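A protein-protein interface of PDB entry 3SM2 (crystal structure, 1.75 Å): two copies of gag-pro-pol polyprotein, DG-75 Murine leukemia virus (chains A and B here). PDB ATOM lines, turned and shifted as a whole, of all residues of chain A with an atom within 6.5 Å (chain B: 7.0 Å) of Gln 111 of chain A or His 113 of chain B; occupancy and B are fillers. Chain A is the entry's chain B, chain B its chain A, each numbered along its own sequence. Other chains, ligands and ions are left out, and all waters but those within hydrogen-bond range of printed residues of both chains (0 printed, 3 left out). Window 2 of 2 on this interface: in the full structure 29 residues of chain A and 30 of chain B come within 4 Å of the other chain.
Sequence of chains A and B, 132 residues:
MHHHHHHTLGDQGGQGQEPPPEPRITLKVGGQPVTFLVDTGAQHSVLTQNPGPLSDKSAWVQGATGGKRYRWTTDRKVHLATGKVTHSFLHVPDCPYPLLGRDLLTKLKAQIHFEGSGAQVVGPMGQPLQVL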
ATOM      1  N   LEU A 105      11.290   4.679  -0.932  1.00  0.00           N
ATOM      2  CA  LEU A 105      12.186   3.535  -0.928  1.00  0.00           C
ATOM      3  C   LEU A 105      12.737   3.333   0.483  1.00  0.00           C
ATOM      4  O   LEU A 105      12.889   2.204   0.926  1.00  0.00           O
ATOM      5  CB  LEU A 105      13.339   3.727  -1.927  1.00  0.00           C
ATOM      6  CG  LEU A 105      12.925   3.559  -3.394  1.00  0.00           C
ATOM      7  CD1 LEU A 105      14.013   4.039  -4.358  1.00  0.00           C
ATOM      8  CD2 LEU A 105      12.555   2.093  -3.668  1.00  0.00           C
ATOM      9  N   LEU A 108       9.906   1.919   2.577  1.00  0.00           N
ATOM     10  CA  LEU A 108       9.729   0.504   2.239  1.00  0.00           C
ATOM     11  C   LEU A 108      10.912  -0.387   2.616  1.00  0.00           C
ATOM     12  O   LEU A 108      10.802  -1.621   2.502  1.00  0.00           O
ATOM     13  CB  LEU A 108       9.454   0.318   0.742  1.00  0.00           C
ATOM     14  CG  LEU A 108       8.025   0.627   0.320  1.00  0.00           C
ATOM     15  CD1 LEU A 108       8.017   0.968  -1.148  1.00  0.00           C
ATOM     16  CD2 LEU A 108       7.090  -0.562   0.629  1.00  0.00           C
ATOM     17  N   LYS A 109      12.020   0.237   3.024  1.00  0.00           N
ATOM     18  CA  LYS A 109      13.312  -0.441   3.235  1.00  0.00           C
ATOM     19  C   LYS A 109      13.637  -1.334   2.038  1.00  0.00           C
ATOM     20  O   LYS A 109      14.029  -2.499   2.181  1.00  0.00           O
ATOM     21  CB  LYS A 109      13.308  -1.235   4.557  1.00  0.00           C
ATOM     22  CG  LYS A 109      13.021  -0.385   5.807  1.00  0.00           C
ATOM     23  CD  LYS A 109      14.086   0.692   5.990  1.00  0.00           C
ATOM     24  CE  LYS A 109      13.689   1.741   7.023  1.00  0.00           C
ATOM     25  NZ  LYS A 109      14.508   2.980   6.838  1.00  0.00           N
ATOM     26  N   ALA A 110      13.465  -0.776   0.843  1.00  0.00           N
ATOM     27  CA  ALA A 110      13.473  -1.594  -0.361  1.00  0.00           C
ATOM     28  C   ALA A 110      14.879  -1.939  -0.826  1.00  0.00           C
ATOM     29  O   ALA A 110      15.848  -1.246  -0.502  1.00  0.00           O
ATOM     30  CB  ALA A 110      12.690  -0.913  -1.500  1.00  0.00           C
ATOM     31  N   GLN A 111      14.963  -3.040  -1.567  1.00  0.00           N
ATOM     32  CA  GLN A 111      16.186  -3.431  -2.284  1.00  0.00           C
ATOM     33  C   GLN A 111      15.900  -3.478  -3.766  1.00  0.00           C
ATOM     34  O   GLN A 111      14.843  -3.978  -4.197  1.00  0.00           O
ATOM     35  CB  GLN A 111      16.657  -4.825  -1.871  1.00  0.00           C
ATOM     36  CG  GLN A 111      16.947  -5.023  -0.412  1.00  0.00           C
ATOM     37  CD  GLN A 111      17.416  -6.443  -0.159  1.00  0.00           C
ATOM     38  OE1 GLN A 111      17.863  -7.134  -1.077  1.00  0.00           O
ATOM     39  NE2 GLN A 111      17.330  -6.883   1.086  1.00  0.00           N
ATOM     40  N   ILE A 112      16.849  -3.004  -4.572  1.00  0.00           N
ATOM     41  CA  ILE A 112      16.683  -3.101  -6.010  1.00  0.00           C
ATOM     42  C   ILE A 112      17.814  -3.984  -6.538  1.00  0.00           C
ATOM     43  O   ILE A 112      18.956  -3.757  -6.206  1.00  0.00           O
ATOM     44  CB  ILE A 112      16.729  -1.692  -6.684  1.00  0.00           C
ATOM     45  CG1 ILE A 112      15.680  -0.761  -6.045  1.00  0.00           C
ATOM     46  CG2 ILE A 112      16.511  -1.805  -8.154  1.00  0.00           C
ATOM     47  CD1 ILE A 112      16.004   0.723  -6.133  1.00  0.00           C
ATOM     48  N   HIS A 113      17.462  -4.978  -7.342  1.00  0.00           N
ATOM     49  CA  HIS A 113      18.418  -5.923  -7.903  1.00  0.00           C
ATOM     50  C   HIS A 113      18.467  -5.890  -9.433  1.00  0.00           C
ATOM     51  O   HIS A 113      17.441  -6.049 -10.087  1.00  0.00           O
ATOM     52  CB  HIS A 113      18.030  -7.327  -7.430  1.00  0.00           C
ATOM     53  CG  HIS A 113      18.177  -7.521  -5.953  1.00  0.00           C
ATOM     54  ND1 HIS A 113      19.096  -8.387  -5.406  1.00  0.00           N
ATOM     55  CD2 HIS A 113      17.529  -6.954  -4.909  1.00  0.00           C
ATOM     56  CE1 HIS A 113      19.010  -8.343  -4.086  1.00  0.00           C
ATOM     57  NE2 HIS A 113      18.063  -7.485  -3.758  1.00  0.00           N
ATOM     58  N   GLN A 120      14.545  -5.956 -10.551  1.00  0.00           N
ATOM     59  CA  GLN A 120      13.448  -6.314  -9.641  1.00  0.00           C
ATOM     60  C   GLN A 120      13.551  -5.576  -8.326  1.00  0.00           C
ATOM     61  O   GLN A 120      14.652  -5.248  -7.886  1.00  0.00           O
ATOM     62  CB  GLN A 120      13.451  -7.820  -9.399  1.00  0.00           C
ATOM     63  CG  GLN A 120      12.571  -8.562 -10.391  1.00  0.00           C
ATOM     64  CD  GLN A 120      13.132  -9.914 -10.813  1.00  0.00           C
ATOM     65  OE1 GLN A 120      13.120 -10.254 -12.004  1.00  0.00           O
ATOM     66  NE2 GLN A 120      13.615 -10.699  -9.843  1.00  0.00           N
ATOM     67  N   VAL A 121      12.403  -5.313  -7.697  1.00  0.00           N
ATOM     68  CA  VAL A 121      12.382  -4.592  -6.422  1.00  0.00           C
ATOM     69  C   VAL A 121      11.763  -5.482  -5.358  1.00  0.00           C
ATOM     70  O   VAL A 121      10.700  -6.063  -5.593  1.00  0.00           O
ATOM     71  CB  VAL A 121      11.549  -3.303  -6.506  1.00  0.00           C
ATOM     72  CG1 VAL A 121      11.911  -2.387  -5.348  1.00  0.00           C
ATOM     73  CG2 VAL A 121      11.789  -2.602  -7.862  1.00  0.00           C
ATOM     74  N   VAL A 122      12.426  -5.574  -4.207  1.00  0.00           N
ATOM     75  CA  VAL A 122      11.992  -6.463  -3.113  1.00  0.00           C
ATOM     76  C   VAL A 122      12.041  -5.729  -1.775  1.00  0.00           C
ATOM     77  O   VAL A 122      12.563  -4.616  -1.695  1.00  0.00           O
ATOM     78  CB  VAL A 122      12.826  -7.787  -3.089  1.00  0.00           C
ATOM     79  CG1 VAL A 122      12.596  -8.581  -4.364  1.00  0.00           C
ATOM     80  CG2 VAL A 122      14.315  -7.511  -2.919  1.00  0.00           C
ATOM     81  N   GLY A 123      11.474  -6.328  -0.726  1.00  0.00           N
ATOM     82  CA  GLY A 123      11.523  -5.727   0.598  1.00  0.00           C
ATOM     83  C   GLY A 123      12.842  -5.915   1.331  1.00  0.00           C
ATOM     84  O   GLY A 123      13.806  -6.469   0.770  1.00  0.00           O
ATOM     85  N   PRO A 124      12.891  -5.456   2.595  1.00  0.00           N
ATOM     86  CA  PRO A 124      14.068  -5.451   3.444  1.00  0.00           C
ATOM     87  C   PRO A 124      14.650  -6.850   3.647  1.00  0.00           C
ATOM     88  O   PRO A 124      15.823  -6.979   3.964  1.00  0.00           O
ATOM     89  CB  PRO A 124      13.547  -4.889   4.775  1.00  0.00           C
ATOM     90  CG  PRO A 124      12.093  -5.031   4.724  1.00  0.00           C
ATOM     91  CD  PRO A 124      11.729  -4.869   3.288  1.00  0.00           C
ATOM     92  N   MET A 125      13.835  -7.879   3.449  1.00  0.00           N
ATOM     93  CA  MET A 125      14.334  -9.245   3.550  1.00  0.00           C
ATOM     94  C   MET A 125      14.120 -10.066   2.291  1.00  0.00           C
ATOM     95  O   MET A 125      13.913 -11.274   2.350  1.00  0.00           O
ATOM     96  CB  MET A 125      13.807  -9.934   4.807  1.00  0.00           C
ATOM     97  CG  MET A 125      14.826  -9.827   5.925  1.00  0.00           C
ATOM     98  SD  MET A 125      14.115  -9.578   7.532  1.00  0.00           S
ATOM     99  CE  MET A 125      13.623  -7.861   7.394  1.00  0.00           C
ATOM    100  N   GLY A 126      14.193  -9.384   1.153  1.00  0.00           N
ATOM    101  CA  GLY A 126      14.306 -10.041  -0.137  1.00  0.00           C
ATOM    102  C   GLY A 126      13.018 -10.548  -0.742  1.00  0.00           C
ATOM    103  O   GLY A 126      13.038 -11.118  -1.834  1.00  0.00           O
ATOM    104  N   LEU A 129       7.689  -7.344  -2.892  1.00  0.00           N
ATOM    105  CA  LEU A 129       6.985  -6.624  -1.818  1.00  0.00           C
ATOM    106  C   LEU A 129       5.573  -7.100  -1.462  1.00  0.00           C
ATOM    107  O   LEU A 129       4.637  -6.967  -2.262  1.00  0.00           O
ATOM    108  CB  LEU A 129       7.059  -5.108  -2.044  1.00  0.00           C
ATOM    109  CG  LEU A 129       8.385  -4.555  -1.501  1.00  0.00           C
ATOM    110  CD1 LEU A 129       8.972  -3.462  -2.375  1.00  0.00           C
ATOM    111  CD2 LEU A 129       8.255  -4.088  -0.041  1.00  0.00           C
ATOM    112  N   GLU B  22      23.126   9.672  -1.281  1.00  0.00           N
ATOM    113  CA  GLU B  22      23.090   8.212  -1.445  1.00  0.00           C
ATOM    114  C   GLU B  22      21.789   7.826  -2.182  1.00  0.00           C
ATOM    115  O   GLU B  22      20.794   8.551  -2.054  1.00  0.00           O
ATOM    116  CB  GLU B  22      23.142   7.529  -0.087  1.00  0.00           C
ATOM    117  CG  GLU B  22      24.447   7.804   0.687  1.00  0.00           C
ATOM    118  CD  GLU B  22      24.543   6.991   1.968  1.00  0.00           C
ATOM    119  OE1 GLU B  22      23.502   6.521   2.475  1.00  0.00           O
ATOM    120  OE2 GLU B  22      25.671   6.814   2.471  1.00  0.00           O
ATOM    121  N   PRO B  23      21.792   6.724  -2.964  1.00  0.00           N
ATOM    122  CA  PRO B  23      22.915   5.826  -3.243  1.00  0.00           C
ATOM    123  C   PRO B  23      23.902   6.492  -4.203  1.00  0.00           C
ATOM    124  O   PRO B  23      23.504   7.037  -5.239  1.00  0.00           O
ATOM    125  CB  PRO B  23      22.250   4.600  -3.893  1.00  0.00           C
ATOM    126  CG  PRO B  23      21.014   5.128  -4.550  1.00  0.00           C
ATOM    127  CD  PRO B  23      20.541   6.278  -3.625  1.00  0.00           C
ATOM    128  N   ALA B 110      24.346  -4.550 -10.132  1.00  0.00           N
ATOM    129  CA  ALA B 110      24.319  -4.000  -8.779  1.00  0.00           C
ATOM    130  C   ALA B 110      23.039  -4.329  -8.011  1.00  0.00           C
ATOM    131  O   ALA B 110      21.972  -4.550  -8.604  1.00  0.00           O
ATOM    132  CB  ALA B 110      24.520  -2.502  -8.820  1.00  0.00           C
ATOM    133  N   GLN B 111      23.159  -4.331  -6.685  1.00  0.00           N
ATOM    134  CA  GLN B 111      21.996  -4.310  -5.790  1.00  0.00           C
ATOM    135  C   GLN B 111      22.051  -3.022  -5.009  1.00  0.00           C
ATOM    136  O   GLN B 111      23.126  -2.541  -4.639  1.00  0.00           O
ATOM    137  CB  GLN B 111      22.022  -5.478  -4.811  1.00  0.00           C
ATOM    138  CG  GLN B 111      22.243  -6.826  -5.444  1.00  0.00           C
ATOM    139  CD  GLN B 111      22.363  -7.926  -4.418  1.00  0.00           C
ATOM    140  OE1 GLN B 111      21.883  -7.795  -3.281  1.00  0.00           O
ATOM    141  NE2 GLN B 111      22.997  -9.026  -4.809  1.00  0.00           N
ATOM    142  N   ILE B 112      20.891  -2.423  -4.796  1.00  0.00           N
ATOM    143  CA  ILE B 112      20.835  -1.189  -4.052  1.00  0.00           C
ATOM    144  C   ILE B 112      19.942  -1.451  -2.850  1.00  0.00           C
ATOM    145  O   ILE B 112      18.792  -1.876  -3.005  1.00  0.00           O
ATOM    146  CB  ILE B 112      20.295  -0.031  -4.925  1.00  0.00           C
ATOM    147  CG1 ILE B 112      21.187   0.159  -6.158  1.00  0.00           C
ATOM    148  CG2 ILE B 112      20.269   1.255  -4.129  1.00  0.00           C
ATOM    149  CD1 ILE B 112      20.423   0.508  -7.419  1.00  0.00           C
ATOM    150  N   HIS B 113      20.487  -1.200  -1.658  1.00  0.00           N
ATOM    151  CA  HIS B 113      19.790  -1.506  -0.398  1.00  0.00           C
ATOM    152  C   HIS B 113      19.464  -0.228   0.363  1.00  0.00           C
ATOM    153  O   HIS B 113      20.369   0.554   0.682  1.00  0.00           O
ATOM    154  CB  HIS B 113      20.669  -2.421   0.471  1.00  0.00           C
ATOM    155  CG  HIS B 113      20.920  -3.770  -0.126  1.00  0.00           C
ATOM    156  ND1 HIS B 113      20.434  -4.930   0.433  1.00  0.00           N
ATOM    157  CD2 HIS B 113      21.618  -4.147  -1.223  1.00  0.00           C
ATOM    158  CE1 HIS B 113      20.815  -5.966  -0.296  1.00  0.00           C
ATOM    159  NE2 HIS B 113      21.529  -5.518  -1.310  1.00  0.00           N
ATOM    160  N   PHE B 114      18.181   0.011   0.617  1.00  0.00           N
ATOM    161  CA  PHE B 114      17.792   1.122   1.486  1.00  0.00           C
ATOM    162  C   PHE B 114      17.694   0.648   2.919  1.00  0.00           C
ATOM    163  O   PHE B 114      16.980  -0.315   3.199  1.00  0.00           O
ATOM    164  CB  PHE B 114      16.499   1.780   1.002  1.00  0.00           C
ATOM    165  CG  PHE B 114      16.704   2.612  -0.234  1.00  0.00           C
ATOM    166  CD1 PHE B 114      16.799   4.005  -0.150  1.00  0.00           C
ATOM    167  CD2 PHE B 114      16.867   1.989  -1.475  1.00  0.00           C
ATOM    168  CE1 PHE B 114      17.014   4.787  -1.292  1.00  0.00           C
ATOM    169  CE2 PHE B 114      17.102   2.767  -2.638  1.00  0.00           C
ATOM    170  CZ  PHE B 114      17.179   4.148  -2.549  1.00  0.00           C
ATOM    171  N   GLU B 115      18.461   1.291   3.800  1.00  0.00           N
ATOM    172  CA  GLU B 115      18.609   0.872   5.207  1.00  0.00           C
ATOM    173  C   GLU B 115      19.026   2.031   6.099  1.00  0.00           C
ATOM    174  O   GLU B 115      20.032   2.699   5.841  1.00  0.00           O
ATOM    175  CB  GLU B 115      19.614  -0.281   5.355  1.00  0.00           C
ATOM    176  CG  GLU B 115      19.033  -1.670   5.085  1.00  0.00           C
ATOM    177  CD  GLU B 115      17.674  -1.881   5.755  1.00  0.00           C
ATOM    178  OE1 GLU B 115      16.764  -2.432   5.094  1.00  0.00           O
ATOM    179  OE2 GLU B 115      17.516  -1.476   6.929  1.00  0.00           O
ATOM    180  N   GLY B 118      19.795   6.076   4.716  1.00  0.00           N
ATOM    181  CA  GLY B 118      20.631   6.085   3.521  1.00  0.00           C
ATOM    182  C   GLY B 118      20.484   4.828   2.682  1.00  0.00           C
ATOM    183  O   GLY B 118      19.539   4.063   2.829  1.00  0.00           O
ATOM    184  N   ALA B 119      21.441   4.603   1.802  1.00  0.00           N
ATOM    185  CA  ALA B 119      21.332   3.534   0.831  1.00  0.00           C
ATOM    186  C   ALA B 119      22.740   3.117   0.467  1.00  0.00           C
ATOM    187  O   ALA B 119      23.615   3.977   0.348  1.00  0.00           O
ATOM    188  CB  ALA B 119      20.582   4.032  -0.421  1.00  0.00           C
ATOM    189  N   GLN B 120      22.946   1.813   0.300  1.00  0.00           N
ATOM    190  CA  GLN B 120      24.259   1.276  -0.059  1.00  0.00           C
ATOM    191  C   GLN B 120      24.202   0.386  -1.297  1.00  0.00           C
ATOM    192  O   GLN B 120      23.203  -0.298  -1.565  1.00  0.00           O
ATOM    193  CB  GLN B 120      24.908   0.547   1.127  1.00  0.00           C
ATOM    194  CG  GLN B 120      24.148  -0.689   1.616  1.00  0.00           C
ATOM    195  CD  GLN B 120      23.992  -0.735   3.137  1.00  0.00           C
ATOM    196  OE1 GLN B 120      22.899  -1.014   3.654  1.00  0.00           O
ATOM    197  NE2 GLN B 120      25.081  -0.455   3.862  1.00  0.00           N
ATOM    198  N   VAL B 121      25.282   0.418  -2.060  1.00  0.00           N
ATOM    199  CA  VAL B 121      25.357  -0.378  -3.272  1.00  0.00           C
ATOM    200  C   VAL B 121      26.222  -1.595  -2.974  1.00  0.00           C
ATOM    201  O   VAL B 121      27.259  -1.465  -2.347  1.00  0.00           O
ATOM    202  CB  VAL B 121      25.991   0.391  -4.446  1.00  0.00           C
ATOM    203  CG1 VAL B 121      25.886  -0.430  -5.745  1.00  0.00           C
ATOM    204  CG2 VAL B 121      25.342   1.796  -4.620  1.00  0.00           C
ATOM    205  N   VAL B 122      25.792  -2.754  -3.462  1.00  0.00           N
ATOM    206  CA  VAL B 122      26.531  -4.005  -3.320  1.00  0.00           C
ATOM    207  C   VAL B 122      26.608  -4.678  -4.698  1.00  0.00           C
ATOM    208  O   VAL B 122      25.784  -4.423  -5.582  1.00  0.00           O
ATOM    209  CB  VAL B 122      25.917  -4.962  -2.224  1.00  0.00           C
ATOM    210  CG1 VAL B 122      25.697  -4.231  -0.889  1.00  0.00           C
ATOM    211  CG2 VAL B 122      24.624  -5.579  -2.691  1.00  0.00           C
ATOM    212  N   GLY B 123      27.617  -5.515  -4.893  1.00  0.00           N
ATOM    213  CA  GLY B 123      27.809  -6.156  -6.183  1.00  0.00           C
ATOM    214  C   GLY B 123      27.050  -7.455  -6.338  1.00  0.00           C
ATOM    215  O   GLY B 123      26.334  -7.893  -5.421  1.00  0.00           O
ATOM    216  N   GLY B 126      27.344 -10.002  -3.688  1.00  0.00           N
ATOM    217  CA  GLY B 126      26.940  -9.524  -2.364  1.00  0.00           C
ATOM    218  C   GLY B 126      28.013  -8.721  -1.656  1.00  0.00           C
ATOM    219  O   GLY B 126      27.836  -8.326  -0.511  1.00  0.00           O
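N of Ile 112 of chain A sits at hydrogen-bond distance from O of Ile 112 of chain B, 2.7 Å away.
N of Phe 114 of chain B is in hydrogen-bond range of O of Ala 110 of chain A, 2.9 Å away.
The backbone NH (N) of His 113 of chain B sits at hydrogen-bond distance from the backbone carbonyl oxygen (O) of Gln 120 of chain B, at 2.9 Å.
O of Leu 105 of chain A sits at hydrogen-bond distance from N of Ala 110 of chain A (3.0 Å).
OE1 of Gln 111 of chain A sits at hydrogen-bond distance from NE2 of His 113 of chain A (2.7 Å).
N of Gln 111 of chain A sits at hydrogen-bond distance from O of Val 122 of chain A (2.9 Å).
The backbone carbonyl oxygen (O) of Pro 124 of chain A lies within hydrogen-bond range of the side-chain amide nitrogen (NE2) of Gln 111 of chain A (3.3 Å).
The backbone NH (N) of His 113 of chain A sits at hydrogen-bond distance from the backbone carbonyl oxygen (O) of Gln 120 of chain A, 2.9 Å away.
Phe 114 of chain B touches Leu 105 of chain A (CB to O, 3.6 Å).
CA of Lys 109 of chain A touches O of Phe 114 of chain B (3.7 Å).
OE1 of Glu 115 of chain B touches CB of Lys 109 of chain A, at 3.7 Å.
O of Ala 110 of chain A touches C of His 113 of chain B, 3.9 Å away.
Ile 112 of chain B touches Gln 111 of chain A.
Gln 111 of chain A touches His 113 of chain B.
O of Ala 110 of chain B touches O of Ile 112 of chain A, 3.9 Å away.
Ile 112 of chain A touches Gln 111 of chain B (O to CA, 3.1 Å).
Ala 110 of chain B touches His 113 of chain A (O to C, 3.8 Å).
His 113 of chain A touches Gln 111 of chain B.
Gln 111 of chain A touches two residues of chain B.
Of the printed residues of chain B, His 113 of chain A touches Ala 110 (3.8 Å) and Gln 111 (3.0 Å).
Printed residues of chain A within 4 Å of Ala 110 of chain B: Ile 112 (3.9 Å) and His 113 (3.8 Å).
Printed residues of chain A within 4 Å of Gln 111 of chain B: Ile 112 (3.1 Å) and His 113 (3.0 Å).
His 113 of chain B touches two residues of chain A.
The nearest residue of chain B that does not touch Gln 111 of chain A is Gln 111 of chain B (4.6 Å).
The nearest residue of chain A that does not touch His 113 of chain B is His 113 of chain A (4.7 Å).
The nearest printed residue of chain B that does not touch His 113 of chain A is His 113 of chain B (4.7 Å).
Of the 15 printed residues of chain A, 6 touch a printed residue of chain B.
Of the 15 printed residues of chain B, 6 touch a printed residue of chain A.
Hydrophobic or aromatic side chains of chain B that line the printed part of chain A: His 113 and Phe 114.
Among the printed residues, 13 pairs touch across the chains.
Ala 110 of chain A touches Ile 112 of chain B, and with the chains exchanged Ile 112 of chain A touches Ala 110 of chain B.
Ala 110 of chain A touches His 113 of chain B, and with the chains exchanged His 113 of chain A touches Ala 110 of chain B.
Gln 111 of chain A touches Ile 112 of chain B, and with the chains exchanged Ile 112 of chain A touches Gln 111 of chain B.
Gln 111 of chain A touches His 113 of chain B, and with the chains exchanged His 113 of chain A touches Gln 111 of chain B.
Positions printed for both chains: 110, 111, 112, 113, 120, 121, 122, 123 and 126.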
